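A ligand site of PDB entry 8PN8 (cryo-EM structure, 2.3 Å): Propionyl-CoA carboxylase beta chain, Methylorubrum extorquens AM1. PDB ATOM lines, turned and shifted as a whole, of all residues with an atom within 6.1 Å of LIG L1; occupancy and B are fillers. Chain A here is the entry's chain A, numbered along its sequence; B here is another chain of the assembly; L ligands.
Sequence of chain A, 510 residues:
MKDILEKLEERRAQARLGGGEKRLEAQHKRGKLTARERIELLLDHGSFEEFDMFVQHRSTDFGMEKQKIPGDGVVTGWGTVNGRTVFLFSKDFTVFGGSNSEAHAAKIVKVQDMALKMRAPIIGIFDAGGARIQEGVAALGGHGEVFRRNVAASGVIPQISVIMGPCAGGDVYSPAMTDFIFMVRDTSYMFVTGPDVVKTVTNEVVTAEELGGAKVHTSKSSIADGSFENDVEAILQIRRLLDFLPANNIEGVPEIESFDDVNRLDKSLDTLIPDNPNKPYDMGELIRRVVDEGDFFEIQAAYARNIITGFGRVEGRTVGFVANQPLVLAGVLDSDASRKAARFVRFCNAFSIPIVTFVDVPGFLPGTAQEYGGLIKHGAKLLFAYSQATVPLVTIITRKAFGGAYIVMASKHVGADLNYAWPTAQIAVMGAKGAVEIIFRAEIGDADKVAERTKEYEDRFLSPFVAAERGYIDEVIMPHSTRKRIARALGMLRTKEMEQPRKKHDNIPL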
ATOM      1  N   ARG A  23     -17.572  -7.109  38.009  1.00  0.00           N
ATOM      2  CA  ARG A  23     -16.398  -6.617  37.286  1.00  0.00           C
ATOM      3  C   ARG A  23     -15.125  -7.294  37.748  1.00  0.00           C
ATOM      4  O   ARG A  23     -14.227  -7.557  36.932  1.00  0.00           O
ATOM      5  CB  ARG A  23     -16.298  -5.098  37.432  1.00  0.00           C
ATOM      6  CG  ARG A  23     -17.406  -4.346  36.726  1.00  0.00           C
ATOM      7  CD  ARG A  23     -17.110  -2.855  36.644  1.00  0.00           C
ATOM      8  NE  ARG A  23     -18.184  -2.108  36.011  1.00  0.00           N
ATOM      9  CZ  ARG A  23     -18.297  -1.912  34.703  1.00  0.00           C
ATOM     10  NH1 ARG A  23     -17.405  -2.408  33.857  1.00  0.00           N
ATOM     11  NH2 ARG A  23     -19.311  -1.202  34.233  1.00  0.00           N
ATOM     12  N   PHE A  93      -8.839  -1.412  36.984  1.00  0.00           N
ATOM     13  CA  PHE A  93      -9.575  -1.460  35.723  1.00  0.00           C
ATOM     14  C   PHE A  93     -11.084  -1.555  35.925  1.00  0.00           C
ATOM     15  O   PHE A  93     -11.844  -1.228  35.007  1.00  0.00           O
ATOM     16  CB  PHE A  93      -9.085  -2.647  34.888  1.00  0.00           C
ATOM     17  CG  PHE A  93      -9.630  -2.677  33.487  1.00  0.00           C
ATOM     18  CD1 PHE A  93      -9.085  -1.850  32.515  1.00  0.00           C
ATOM     19  CD2 PHE A  93     -10.677  -3.508  33.146  1.00  0.00           C
ATOM     20  CE1 PHE A  93      -9.582  -1.877  31.224  1.00  0.00           C
ATOM     21  CE2 PHE A  93     -11.170  -3.530  31.864  1.00  0.00           C
ATOM     22  CZ  PHE A  93     -10.624  -2.713  30.896  1.00  0.00           C
ATOM     23  N   PHE A  96     -14.322   2.772  36.600  1.00  0.00           N
ATOM     24  CA  PHE A  96     -14.305   3.701  35.472  1.00  0.00           C
ATOM     25  C   PHE A  96     -13.279   3.287  34.415  1.00  0.00           C
ATOM     26  O   PHE A  96     -12.745   4.128  33.683  1.00  0.00           O
ATOM     27  CB  PHE A  96     -14.040   5.143  35.916  1.00  0.00           C
ATOM     28  CG  PHE A  96     -15.082   5.680  36.865  1.00  0.00           C
ATOM     29  CD1 PHE A  96     -16.349   5.998  36.412  1.00  0.00           C
ATOM     30  CD2 PHE A  96     -14.775   5.878  38.206  1.00  0.00           C
ATOM     31  CE1 PHE A  96     -17.296   6.494  37.281  1.00  0.00           C
ATOM     32  CE2 PHE A  96     -15.723   6.374  39.075  1.00  0.00           C
ATOM     33  CZ  PHE A  96     -16.983   6.686  38.610  1.00  0.00           C
ATOM     34  N   GLY A  97     -13.005   1.983  34.321  1.00  0.00           N
ATOM     35  CA  GLY A  97     -12.013   1.508  33.384  1.00  0.00           C
ATOM     36  C   GLY A  97     -10.584   1.862  33.733  1.00  0.00           C
ATOM     37  O   GLY A  97      -9.706   1.748  32.881  1.00  0.00           O
ATOM     38  N   GLY A  98     -10.327   2.297  34.967  1.00  0.00           N
ATOM     39  CA  GLY A  98      -9.004   2.740  35.337  1.00  0.00           C
ATOM     40  C   GLY A  98      -8.610   4.087  34.793  1.00  0.00           C
ATOM     41  O   GLY A  98      -7.447   4.473  34.911  1.00  0.00           O
ATOM     42  N   SER A  99      -9.547   4.820  34.193  1.00  0.00           N
ATOM     43  CA  SER A  99      -9.221   6.056  33.507  1.00  0.00           C
ATOM     44  C   SER A  99      -8.722   7.125  34.478  1.00  0.00           C
ATOM     45  O   SER A  99      -9.219   7.242  35.601  1.00  0.00           O
ATOM     46  CB  SER A  99     -10.432   6.572  32.742  1.00  0.00           C
ATOM     47  OG  SER A  99     -11.551   6.708  33.600  1.00  0.00           O
ATOM     48  N   ALA A 128      -5.608   0.347  32.505  1.00  0.00           N
ATOM     49  CA  ALA A 128      -6.487   1.504  32.466  1.00  0.00           C
ATOM     50  C   ALA A 128      -7.031   1.687  31.059  1.00  0.00           C
ATOM     51  O   ALA A 128      -6.903   0.811  30.200  1.00  0.00           O
ATOM     52  CB  ALA A 128      -5.729   2.757  32.946  1.00  0.00           C
ATOM     53  N   GLY A 129      -7.668   2.833  30.823  1.00  0.00           N
ATOM     54  CA  GLY A 129      -8.241   3.162  29.544  1.00  0.00           C
ATOM     55  C   GLY A 129      -8.014   4.611  29.151  1.00  0.00           C
ATOM     56  O   GLY A 129      -8.855   5.206  28.462  1.00  0.00           O
ATOM     57  N   GLY A 130      -6.903   5.188  29.588  1.00  0.00           N
ATOM     58  CA  GLY A 130      -6.580   6.557  29.233  1.00  0.00           C
ATOM     59  C   GLY A 130      -7.081   7.577  30.246  1.00  0.00           C
ATOM     60  O   GLY A 130      -7.020   7.339  31.455  1.00  0.00           O
ATOM     61  N   ALA A 131      -7.583   8.713  29.753  1.00  0.00           N
ATOM     62  CA  ALA A 131      -8.134   9.760  30.604  1.00  0.00           C
ATOM     63  C   ALA A 131      -9.649   9.793  30.472  1.00  0.00           C
ATOM     64  O   ALA A 131     -10.208   9.476  29.426  1.00  0.00           O
ATOM     65  CB  ALA A 131      -7.550  11.133  30.231  1.00  0.00           C
ATOM     66  N   ARG A 132     -10.300  10.198  31.567  1.00  0.00           N
ATOM     67  CA  ARG A 132     -11.757  10.205  31.619  1.00  0.00           C
ATOM     68  C   ARG A 132     -12.305  11.341  30.768  1.00  0.00           C
ATOM     69  O   ARG A 132     -11.940  12.501  30.957  1.00  0.00           O
ATOM     70  CB  ARG A 132     -12.227  10.334  33.064  1.00  0.00           C
ATOM     71  CG  ARG A 132     -13.594   9.757  33.356  1.00  0.00           C
ATOM     72  CD  ARG A 132     -13.780   9.584  34.842  1.00  0.00           C
ATOM     73  NE  ARG A 132     -12.734   8.766  35.428  1.00  0.00           N
ATOM     74  CZ  ARG A 132     -12.583   8.555  36.729  1.00  0.00           C
ATOM     75  NH1 ARG A 132     -13.397   9.109  37.618  1.00  0.00           N
ATOM     76  NH2 ARG A 132     -11.588   7.773  37.148  1.00  0.00           N
ATOM     77  N   ILE A 133     -13.186  11.005  29.822  1.00  0.00           N
ATOM     78  CA  ILE A 133     -13.682  12.002  28.878  1.00  0.00           C
ATOM     79  C   ILE A 133     -14.595  13.004  29.568  1.00  0.00           C
ATOM     80  O   ILE A 133     -14.556  14.201  29.282  1.00  0.00           O
ATOM     81  CB  ILE A 133     -14.383  11.314  27.691  1.00  0.00           C
ATOM     82  CG1 ILE A 133     -13.431  10.330  27.011  1.00  0.00           C
ATOM     83  CG2 ILE A 133     -14.853  12.344  26.682  1.00  0.00           C
ATOM     84  CD1 ILE A 133     -12.170  10.978  26.471  1.00  0.00           C
ATOM     85  N   GLN A 134     -15.444  12.519  30.487  1.00  0.00           N
ATOM     86  CA  GLN A 134     -16.380  13.401  31.167  1.00  0.00           C
ATOM     87  C   GLN A 134     -15.689  14.406  32.077  1.00  0.00           C
ATOM     88  O   GLN A 134     -16.270  15.468  32.362  1.00  0.00           O
ATOM     89  CB  GLN A 134     -17.388  12.572  31.976  1.00  0.00           C
ATOM     90  CG  GLN A 134     -18.319  11.697  31.147  1.00  0.00           C
ATOM     91  CD  GLN A 134     -17.686  10.394  30.727  1.00  0.00           C
ATOM     92  OE1 GLN A 134     -16.513  10.131  31.033  1.00  0.00           O
ATOM     93  NE2 GLN A 134     -18.446   9.560  30.034  1.00  0.00           N
ATOM     94  N   PRO A 166      -4.626  -2.620  29.212  1.00  0.00           N
ATOM     95  CA  PRO A 166      -4.612  -1.562  28.198  1.00  0.00           C
ATOM     96  C   PRO A 166      -3.944  -0.289  28.718  1.00  0.00           C
ATOM     97  O   PRO A 166      -4.013   0.033  29.898  1.00  0.00           O
ATOM     98  CB  PRO A 166      -6.098  -1.325  27.896  1.00  0.00           C
ATOM     99  CG  PRO A 166      -6.765  -2.584  28.315  1.00  0.00           C
ATOM    100  CD  PRO A 166      -5.992  -3.094  29.485  1.00  0.00           C
ATOM    101  N   CYS A 167      -3.293   0.420  27.800  1.00  0.00           N
ATOM    102  CA  CYS A 167      -2.640   1.689  28.122  1.00  0.00           C
ATOM    103  C   CYS A 167      -2.639   2.512  26.839  1.00  0.00           C
ATOM    104  O   CYS A 167      -1.846   2.246  25.937  1.00  0.00           O
ATOM    105  CB  CYS A 167      -1.239   1.478  28.666  1.00  0.00           C
ATOM    106  SG  CYS A 167      -0.405   2.970  29.252  1.00  0.00           S
ATOM    107  N   ALA A 168      -3.530   3.488  26.757  1.00  0.00           N
ATOM    108  CA  ALA A 168      -3.743   4.227  25.514  1.00  0.00           C
ATOM    109  C   ALA A 168      -3.831   5.717  25.781  1.00  0.00           C
ATOM    110  O   ALA A 168      -4.091   6.156  26.908  1.00  0.00           O
ATOM    111  CB  ALA A 168      -5.008   3.748  24.799  1.00  0.00           C
ATOM    112  N   GLY A 169      -3.600   6.495  24.727  1.00  0.00           N
ATOM    113  CA  GLY A 169      -3.720   7.940  24.825  1.00  0.00           C
ATOM    114  C   GLY A 169      -2.560   8.559  25.572  1.00  0.00           C
ATOM    115  O   GLY A 169      -1.385   8.223  25.357  1.00  0.00           O
ATOM    116  N   GLY A 170      -2.880   9.488  26.472  1.00  0.00           N
ATOM    117  CA  GLY A 170      -1.862  10.123  27.295  1.00  0.00           C
ATOM    118  C   GLY A 170      -1.335   9.267  28.417  1.00  0.00           C
ATOM    119  O   GLY A 170      -0.386   9.664  29.094  1.00  0.00           O
ATOM    120  N   TYR A 189      -1.324  -3.854  26.197  1.00  0.00           N
ATOM    121  CA  TYR A 189      -0.888  -3.191  24.983  1.00  0.00           C
ATOM    122  C   TYR A 189      -0.741  -1.700  25.246  1.00  0.00           C
ATOM    123  O   TYR A 189      -1.380  -1.149  26.147  1.00  0.00           O
ATOM    124  CB  TYR A 189      -1.859  -3.439  23.822  1.00  0.00           C
ATOM    125  CG  TYR A 189      -3.318  -3.293  24.177  1.00  0.00           C
ATOM    126  CD1 TYR A 189      -3.924  -2.051  24.205  1.00  0.00           C
ATOM    127  CD2 TYR A 189      -4.094  -4.412  24.458  1.00  0.00           C
ATOM    128  CE1 TYR A 189      -5.262  -1.917  24.513  1.00  0.00           C
ATOM    129  CE2 TYR A 189      -5.431  -4.286  24.772  1.00  0.00           C
ATOM    130  CZ  TYR A 189      -6.003  -3.031  24.802  1.00  0.00           C
ATOM    131  OH  TYR A 189      -7.340  -2.906  25.115  1.00  0.00           O
ATOM    132  N   PHE A 191      -0.312   2.151  23.104  1.00  0.00           N
ATOM    133  CA  PHE A 191      -0.238   2.986  21.905  1.00  0.00           C
ATOM    134  C   PHE A 191      -0.783   4.366  22.233  1.00  0.00           C
ATOM    135  O   PHE A 191      -1.668   4.512  23.082  1.00  0.00           O
ATOM    136  CB  PHE A 191      -1.007   2.372  20.733  1.00  0.00           C
ATOM    137  CG  PHE A 191      -2.275   1.676  21.119  1.00  0.00           C
ATOM    138  CD1 PHE A 191      -3.378   2.398  21.545  1.00  0.00           C
ATOM    139  CD2 PHE A 191      -2.379   0.296  21.021  1.00  0.00           C
ATOM    140  CE1 PHE A 191      -4.543   1.753  21.896  1.00  0.00           C
ATOM    141  CE2 PHE A 191      -3.547  -0.345  21.360  1.00  0.00           C
ATOM    142  CZ  PHE A 191      -4.621   0.379  21.809  1.00  0.00           C
ATOM    143  N   VAL A 192      -0.233   5.375  21.561  1.00  0.00           N
ATOM    144  CA  VAL A 192      -0.728   6.731  21.735  1.00  0.00           C
ATOM    145  C   VAL A 192      -2.110   6.881  21.119  1.00  0.00           C
ATOM    146  O   VAL A 192      -2.983   7.562  21.675  1.00  0.00           O
ATOM    147  CB  VAL A 192       0.269   7.746  21.147  1.00  0.00           C
ATOM    148  CG1 VAL A 192      -0.176   9.164  21.437  1.00  0.00           C
ATOM    149  CG2 VAL A 192       1.667   7.504  21.697  1.00  0.00           C
ATOM    150  N   THR A 193      -2.336   6.265  19.970  1.00  0.00           N
ATOM    151  CA  THR A 193      -3.594   6.359  19.245  1.00  0.00           C
ATOM    152  C   THR A 193      -4.194   4.968  19.075  1.00  0.00           C
ATOM    153  O   THR A 193      -3.476   4.014  18.734  1.00  0.00           O
ATOM    154  CB  THR A 193      -3.401   7.018  17.883  1.00  0.00           C
ATOM    155  OG1 THR A 193      -2.716   8.274  18.053  1.00  0.00           O
ATOM    156  CG2 THR A 193      -4.731   7.275  17.211  1.00  0.00           C
ATOM    157  N   GLY A 194      -5.486   4.848  19.331  1.00  0.00           N
ATOM    158  CA  GLY A 194      -6.155   3.562  19.317  1.00  0.00           C
ATOM    159  C   GLY A 194      -6.463   3.076  17.926  1.00  0.00           C
ATOM    160  O   GLY A 194      -6.360   3.804  16.930  1.00  0.00           O
ATOM    161  N   PRO A 195      -6.844   1.793  17.847  1.00  0.00           N
ATOM    162  CA  PRO A 195      -7.125   1.198  16.527  1.00  0.00           C
ATOM    163  C   PRO A 195      -8.265   1.857  15.775  1.00  0.00           C
ATOM    164  O   PRO A 195      -8.218   1.911  14.535  1.00  0.00           O
ATOM    165  CB  PRO A 195      -7.464  -0.263  16.878  1.00  0.00           C
ATOM    166  CG  PRO A 195      -6.820  -0.493  18.194  1.00  0.00           C
ATOM    167  CD  PRO A 195      -6.912   0.801  18.921  1.00  0.00           C
ATOM    168  N   ASP A 196      -9.283   2.359  16.465  1.00  0.00           N
ATOM    169  CA  ASP A 196     -10.416   2.965  15.762  1.00  0.00           C
ATOM    170  C   ASP A 196      -9.998   4.241  15.040  1.00  0.00           C
ATOM    171  O   ASP A 196     -10.386   4.459  13.887  1.00  0.00           O
ATOM    172  CB  ASP A 196     -11.566   3.243  16.739  1.00  0.00           C
ATOM    173  CG  ASP A 196     -11.181   4.236  17.824  1.00  0.00           C
ATOM    174  OD1 ASP A 196      -9.997   4.265  18.209  1.00  0.00           O
ATOM    175  OD2 ASP A 196     -12.064   4.981  18.288  1.00  0.00           O
ATOM    176  N   VAL A 197      -9.208   5.086  15.690  1.00  0.00           N
ATOM    177  CA  VAL A 197      -8.732   6.311  15.042  1.00  0.00           C
ATOM    178  C   VAL A 197      -7.771   5.972  13.913  1.00  0.00           C
ATOM    179  O   VAL A 197      -7.739   6.659  12.884  1.00  0.00           O
ATOM    180  CB  VAL A 197      -8.092   7.241  16.088  1.00  0.00           C
ATOM    181  CG1 VAL A 197      -7.712   8.572  15.449  1.00  0.00           C
ATOM    182  CG2 VAL A 197      -9.039   7.463  17.251  1.00  0.00           C
ATOM    183  N   ALA A 208      -5.715  -4.356  18.722  1.00  0.00           N
ATOM    184  CA  ALA A 208      -4.899  -3.799  19.808  1.00  0.00           C
ATOM    185  C   ALA A 208      -3.580  -4.541  19.932  1.00  0.00           C
ATOM    186  O   ALA A 208      -2.523  -3.923  20.128  1.00  0.00           O
ATOM    187  CB  ALA A 208      -5.681  -3.847  21.118  1.00  0.00           C
ATOM    188  N   MET B 430     -10.536  16.213  23.259  1.00  0.00           N
ATOM    189  CA  MET B 430     -10.579  15.813  21.852  1.00  0.00           C
ATOM    190  C   MET B 430     -11.604  16.689  21.141  1.00  0.00           C
ATOM    191  O   MET B 430     -12.123  17.648  21.721  1.00  0.00           O
ATOM    192  CB  MET B 430     -10.897  14.318  21.715  1.00  0.00           C
ATOM    193  CG  MET B 430     -12.214  13.900  22.325  1.00  0.00           C
ATOM    194  SD  MET B 430     -12.551  12.145  22.104  1.00  0.00           S
ATOM    195  CE  MET B 430     -11.130  11.434  22.922  1.00  0.00           C
ATOM    196  N   ILE B 438     -17.938   9.061  22.308  1.00  0.00           N
ATOM    197  CA  ILE B 438     -17.510   8.294  23.473  1.00  0.00           C
ATOM    198  C   ILE B 438     -18.509   8.437  24.616  1.00  0.00           C
ATOM    199  O   ILE B 438     -18.869   7.443  25.271  1.00  0.00           O
ATOM    200  CB  ILE B 438     -16.090   8.707  23.891  1.00  0.00           C
ATOM    201  CG1 ILE B 438     -15.088   8.363  22.795  1.00  0.00           C
ATOM    202  CG2 ILE B 438     -15.706   8.027  25.198  1.00  0.00           C
ATOM    203  CD1 ILE B 438     -13.668   8.727  23.142  1.00  0.00           C
ATOM    204  N   ARG B 441     -22.467   7.097  23.762  1.00  0.00           N
ATOM    205  CA  ARG B 441     -22.305   5.911  22.935  1.00  0.00           C
ATOM    206  C   ARG B 441     -23.579   5.090  22.833  1.00  0.00           C
ATOM    207  O   ARG B 441     -23.732   4.319  21.881  1.00  0.00           O
ATOM    208  CB  ARG B 441     -21.157   5.052  23.463  1.00  0.00           C
ATOM    209  CG  ARG B 441     -21.243   4.778  24.949  1.00  0.00           C
ATOM    210  CD  ARG B 441     -19.996   4.077  25.471  1.00  0.00           C
ATOM    211  NE  ARG B 441     -20.023   3.918  26.916  1.00  0.00           N
ATOM    212  CZ  ARG B 441     -19.600   4.825  27.776  1.00  0.00           C
ATOM    213  NH1 ARG B 441     -19.104   5.979  27.377  1.00  0.00           N
ATOM    214  NH2 ARG B 441     -19.671   4.557  29.082  1.00  0.00           N
HETATM  215  N1  LIG L   1     -12.479   7.576  29.813  1.00  0.00           N
HETATM  216  C1  LIG L   1     -13.585   7.184  30.403  1.00  0.00           C
HETATM  217  N2  LIG L   1     -13.964   5.920  30.446  1.00  0.00           N
HETATM  218  C2  LIG L   1     -13.213   4.981  29.876  1.00  0.00           C
HETATM  219  C3  LIG L   1     -12.025   5.353  29.225  1.00  0.00           C
HETATM  220  C4  LIG L   1     -11.673   6.713  29.214  1.00  0.00           C
HETATM  221  N3  LIG L   1     -10.508   7.135  28.594  1.00  0.00           N
HETATM  222  N4  LIG L   1     -11.472   4.217  28.737  1.00  0.00           N
HETATM  223  C5  LIG L   1     -12.215   3.198  29.036  1.00  0.00           C
HETATM  224  N5  LIG L   1     -13.309   3.620  29.728  1.00  0.00           N
HETATM  225  C6  LIG L   1     -14.380   2.757  30.242  1.00  0.00           C
HETATM  226  C7  LIG L   1     -15.405   2.437  29.118  1.00  0.00           C
HETATM  227  O1  LIG L   1     -16.491   3.375  29.140  1.00  0.00           O
HETATM  228  C8  LIG L   1     -15.894   1.028  29.506  1.00  0.00           C
HETATM  229  O2  LIG L   1     -17.008   1.115  30.400  1.00  0.00           O
HETATM  230  P1  LIG L   1     -17.912  -0.209  30.216  1.00  0.00           P
HETATM  231  O3  LIG L   1     -18.151  -0.445  28.781  1.00  0.00           O
HETATM  232  O4  LIG L   1     -17.177  -1.484  30.866  1.00  0.00           O
HETATM  233  O5  LIG L   1     -19.323   0.019  30.955  1.00  0.00           O
HETATM  234  C9  LIG L   1     -14.670   0.407  30.201  1.00  0.00           C
HETATM  235  O6  LIG L   1     -13.806   1.478  30.612  1.00  0.00           O
HETATM  236  C10 LIG L   1     -13.919  -0.539  29.258  1.00  0.00           C
HETATM  237  O7  LIG L   1     -13.723   0.079  27.990  1.00  0.00           O
HETATM  238  P2  LIG L   1     -13.514  -1.100  26.920  1.00  0.00           P
HETATM  239  O8  LIG L   1     -13.385  -0.517  25.566  1.00  0.00           O
HETATM  240  O9  LIG L   1     -14.799  -2.075  26.954  1.00  0.00           O
HETATM  241  O10 LIG L   1     -12.204  -1.944  27.322  1.00  0.00           O
HETATM  242  P3  LIG L   1     -11.123  -1.925  26.118  1.00  0.00           P
HETATM  243  O11 LIG L   1      -9.921  -2.661  26.556  1.00  0.00           O
HETATM  244  O12 LIG L   1     -11.740  -2.641  24.813  1.00  0.00           O
HETATM  245  O13 LIG L   1     -10.696  -0.415  25.751  1.00  0.00           O
HETATM  246  C11 LIG L   1      -8.774   0.901  25.064  1.00  0.00           C
HETATM  247  C12 LIG L   1      -9.271  -0.364  25.766  1.00  0.00           C
HETATM  248  C13 LIG L   1      -7.744   1.596  25.958  1.00  0.00           C
HETATM  249  C14 LIG L   1      -8.117   0.496  23.736  1.00  0.00           C
HETATM  250  C15 LIG L   1      -9.958   1.842  24.798  1.00  0.00           C
HETATM  251  O14 LIG L   1     -10.822   1.837  25.938  1.00  0.00           O
HETATM  252  C16 LIG L   1      -9.511   3.260  24.534  1.00  0.00           C
HETATM  253  O15 LIG L   1      -8.837   3.519  23.557  1.00  0.00           O
HETATM  254  N6  LIG L   1      -9.879   4.243  25.388  1.00  0.00           N
HETATM  255  C17 LIG L   1      -9.481   5.635  25.183  1.00  0.00           C
HETATM  256  C18 LIG L   1      -7.981   5.829  25.441  1.00  0.00           C
HETATM  257  C19 LIG L   1      -7.340   6.540  24.272  1.00  0.00           C
HETATM  258  O16 LIG L   1      -7.048   7.706  24.367  1.00  0.00           O
HETATM  259  N7  LIG L   1      -7.079   5.861  23.140  1.00  0.00           N
HETATM  260  C20 LIG L   1      -6.453   6.544  22.004  1.00  0.00           C
HETATM  261  C21 LIG L   1      -7.521   7.045  21.039  1.00  0.00           C
HETATM  262  S1  LIG L   1      -6.886   8.482  20.124  1.00  0.00           S
HETATM  263  C1  LG2 L   2     -11.936  13.124  11.324  1.00  0.00           C
HETATM  264  O1  LG2 L   2     -11.474  12.388  10.465  1.00  0.00           O
HETATM  265  C2  LG2 L   2     -11.444  13.049  12.744  1.00  0.00           C
HETATM  266  C3  LG2 L   2     -10.242  12.119  12.838  1.00  0.00           C
HETATM  267  C4  LG2 L   2      -8.953  12.898  12.628  1.00  0.00           C
HETATM  268  C5  LG2 L   2      -8.454  13.469  13.940  1.00  0.00           C
HETATM  269  C6  LG2 L   2      -7.068  14.071  13.820  1.00  0.00           C
HETATM  270  S1  LG2 L   2      -5.941  12.970  12.896  1.00  0.00           S
HETATM  271  C7  LG2 L   2      -4.461  13.519  13.737  1.00  0.00           C
HETATM  272  C8  LG2 L   2      -4.861  13.949  15.148  1.00  0.00           C
HETATM  273  N1  LG2 L   2      -4.693  12.832  16.067  1.00  0.00           N
HETATM  274  C9  LG2 L   2      -5.906  12.411  16.670  1.00  0.00           C
HETATM  275  O2  LG2 L   2      -6.073  11.510  17.472  1.00  0.00           O
HETATM  276  N2  LG2 L   2      -6.908  13.248  16.140  1.00  0.00           N
HETATM  277  C10 LG2 L   2      -6.430  14.249  15.200  1.00  0.00           C
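Phe 93 touches LIG L1. Phe 96 touches LIG L1 (O to N2, 3.9 Å). Gly 97 touches LIG L1 (CA to O6, 3.3 Å). Ser 99 touches LIG L1 (CB to N1, 3.7 Å). Gly 130 touches LIG L1. CA of Arg 132 touches N1 of LIG L1 (3.3 Å). Ile 133 touches LIG L1 (N to N1, 3.5 Å). Pro 166 touches LIG L1 (CG to O11, 3.6 Å). CB of Ala 168 touches N7 of LIG L1 (3.4 Å). Gly 169 touches LIG L1 (CA to O16, 3.4 Å). CZ of Phe 191 touches C14 of LIG L1, at 3.99 Å. Val 192 touches LIG L1. Thr 193 touches LIG L1. Gly 194 touches LIG L1 (N to C20, 3.3 Å). Val 197 touches LIG L1. Hydrophobic or aromatic side chains within 4 Å of LIG L1: Phe 93, Pro 166, Ala 168, Tyr 189, Phe 191 and Val 197. 20 residues have an atom within 4 Å of LIG L1: Arg 23, Phe 93, Phe 96, Gly 97, Ser 99, Gly 129, Gly 130, Ala 131, Arg 132, Ile 133, Pro 166, Ala 168, Gly 169, Tyr 189, Phe 191, Val 192, Thr 193, Gly 194, Val 197 and Arg 441 of chain B. The nearest printed residue that does not touch LIG L1 is Gln 134 (4.2 Å).
An oxygen (O1) of LIG L1 sits at hydrogen-bond distance from the guanidinium group (NH2) of Arg 441 of chain B. O4 of LIG L1 is in salt-bridge range of NH1 of Arg 23 (3.1 Å). The backbone carbonyl oxygen (O) of Gly 129 is in hydrogen-bond range of a nitrogen (N3) of LIG L1, 2.5 Å away. N3 of LIG L1 lies within hydrogen-bond range of O of Ala 131, 2.5 Å away. The side-chain hydroxyl (OH) of Tyr 189 lies within hydrogen-bond range of an oxygen (O11) of LIG L1, at 3.0 Å.
The backbone NH (N) of Gly 129 lies within hydrogen-bond range of the backbone carbonyl oxygen (O) of Gly 97, 3.1 Å away. The backbone carbonyl oxygen of Val 192 sits close to the backbone NH of Gly 169 (3.3 Å). NH2 of Arg 132 is in hydrogen-bond range of O of Ser 99, 2.9 Å away. N of Cys 167 is in hydrogen-bond range of O of Tyr 189 (3.0 Å). The guanidinium group (NH1) of Arg 441 of chain B is in hydrogen-bond range of the backbone carbonyl oxygen (O) of Ile 438 of chain B (2.6 Å). O of Cys 167 lies within hydrogen-bond range of N of Phe 191 (3.2 Å). N of Ala 128 sits at hydrogen-bond distance from O of Pro 166 (3.1 Å). The side-chain hydroxyl (OG) of Ser 99 sits at hydrogen-bond distance from the backbone carbonyl oxygen (O) of Phe 96, at 2.8 Å.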
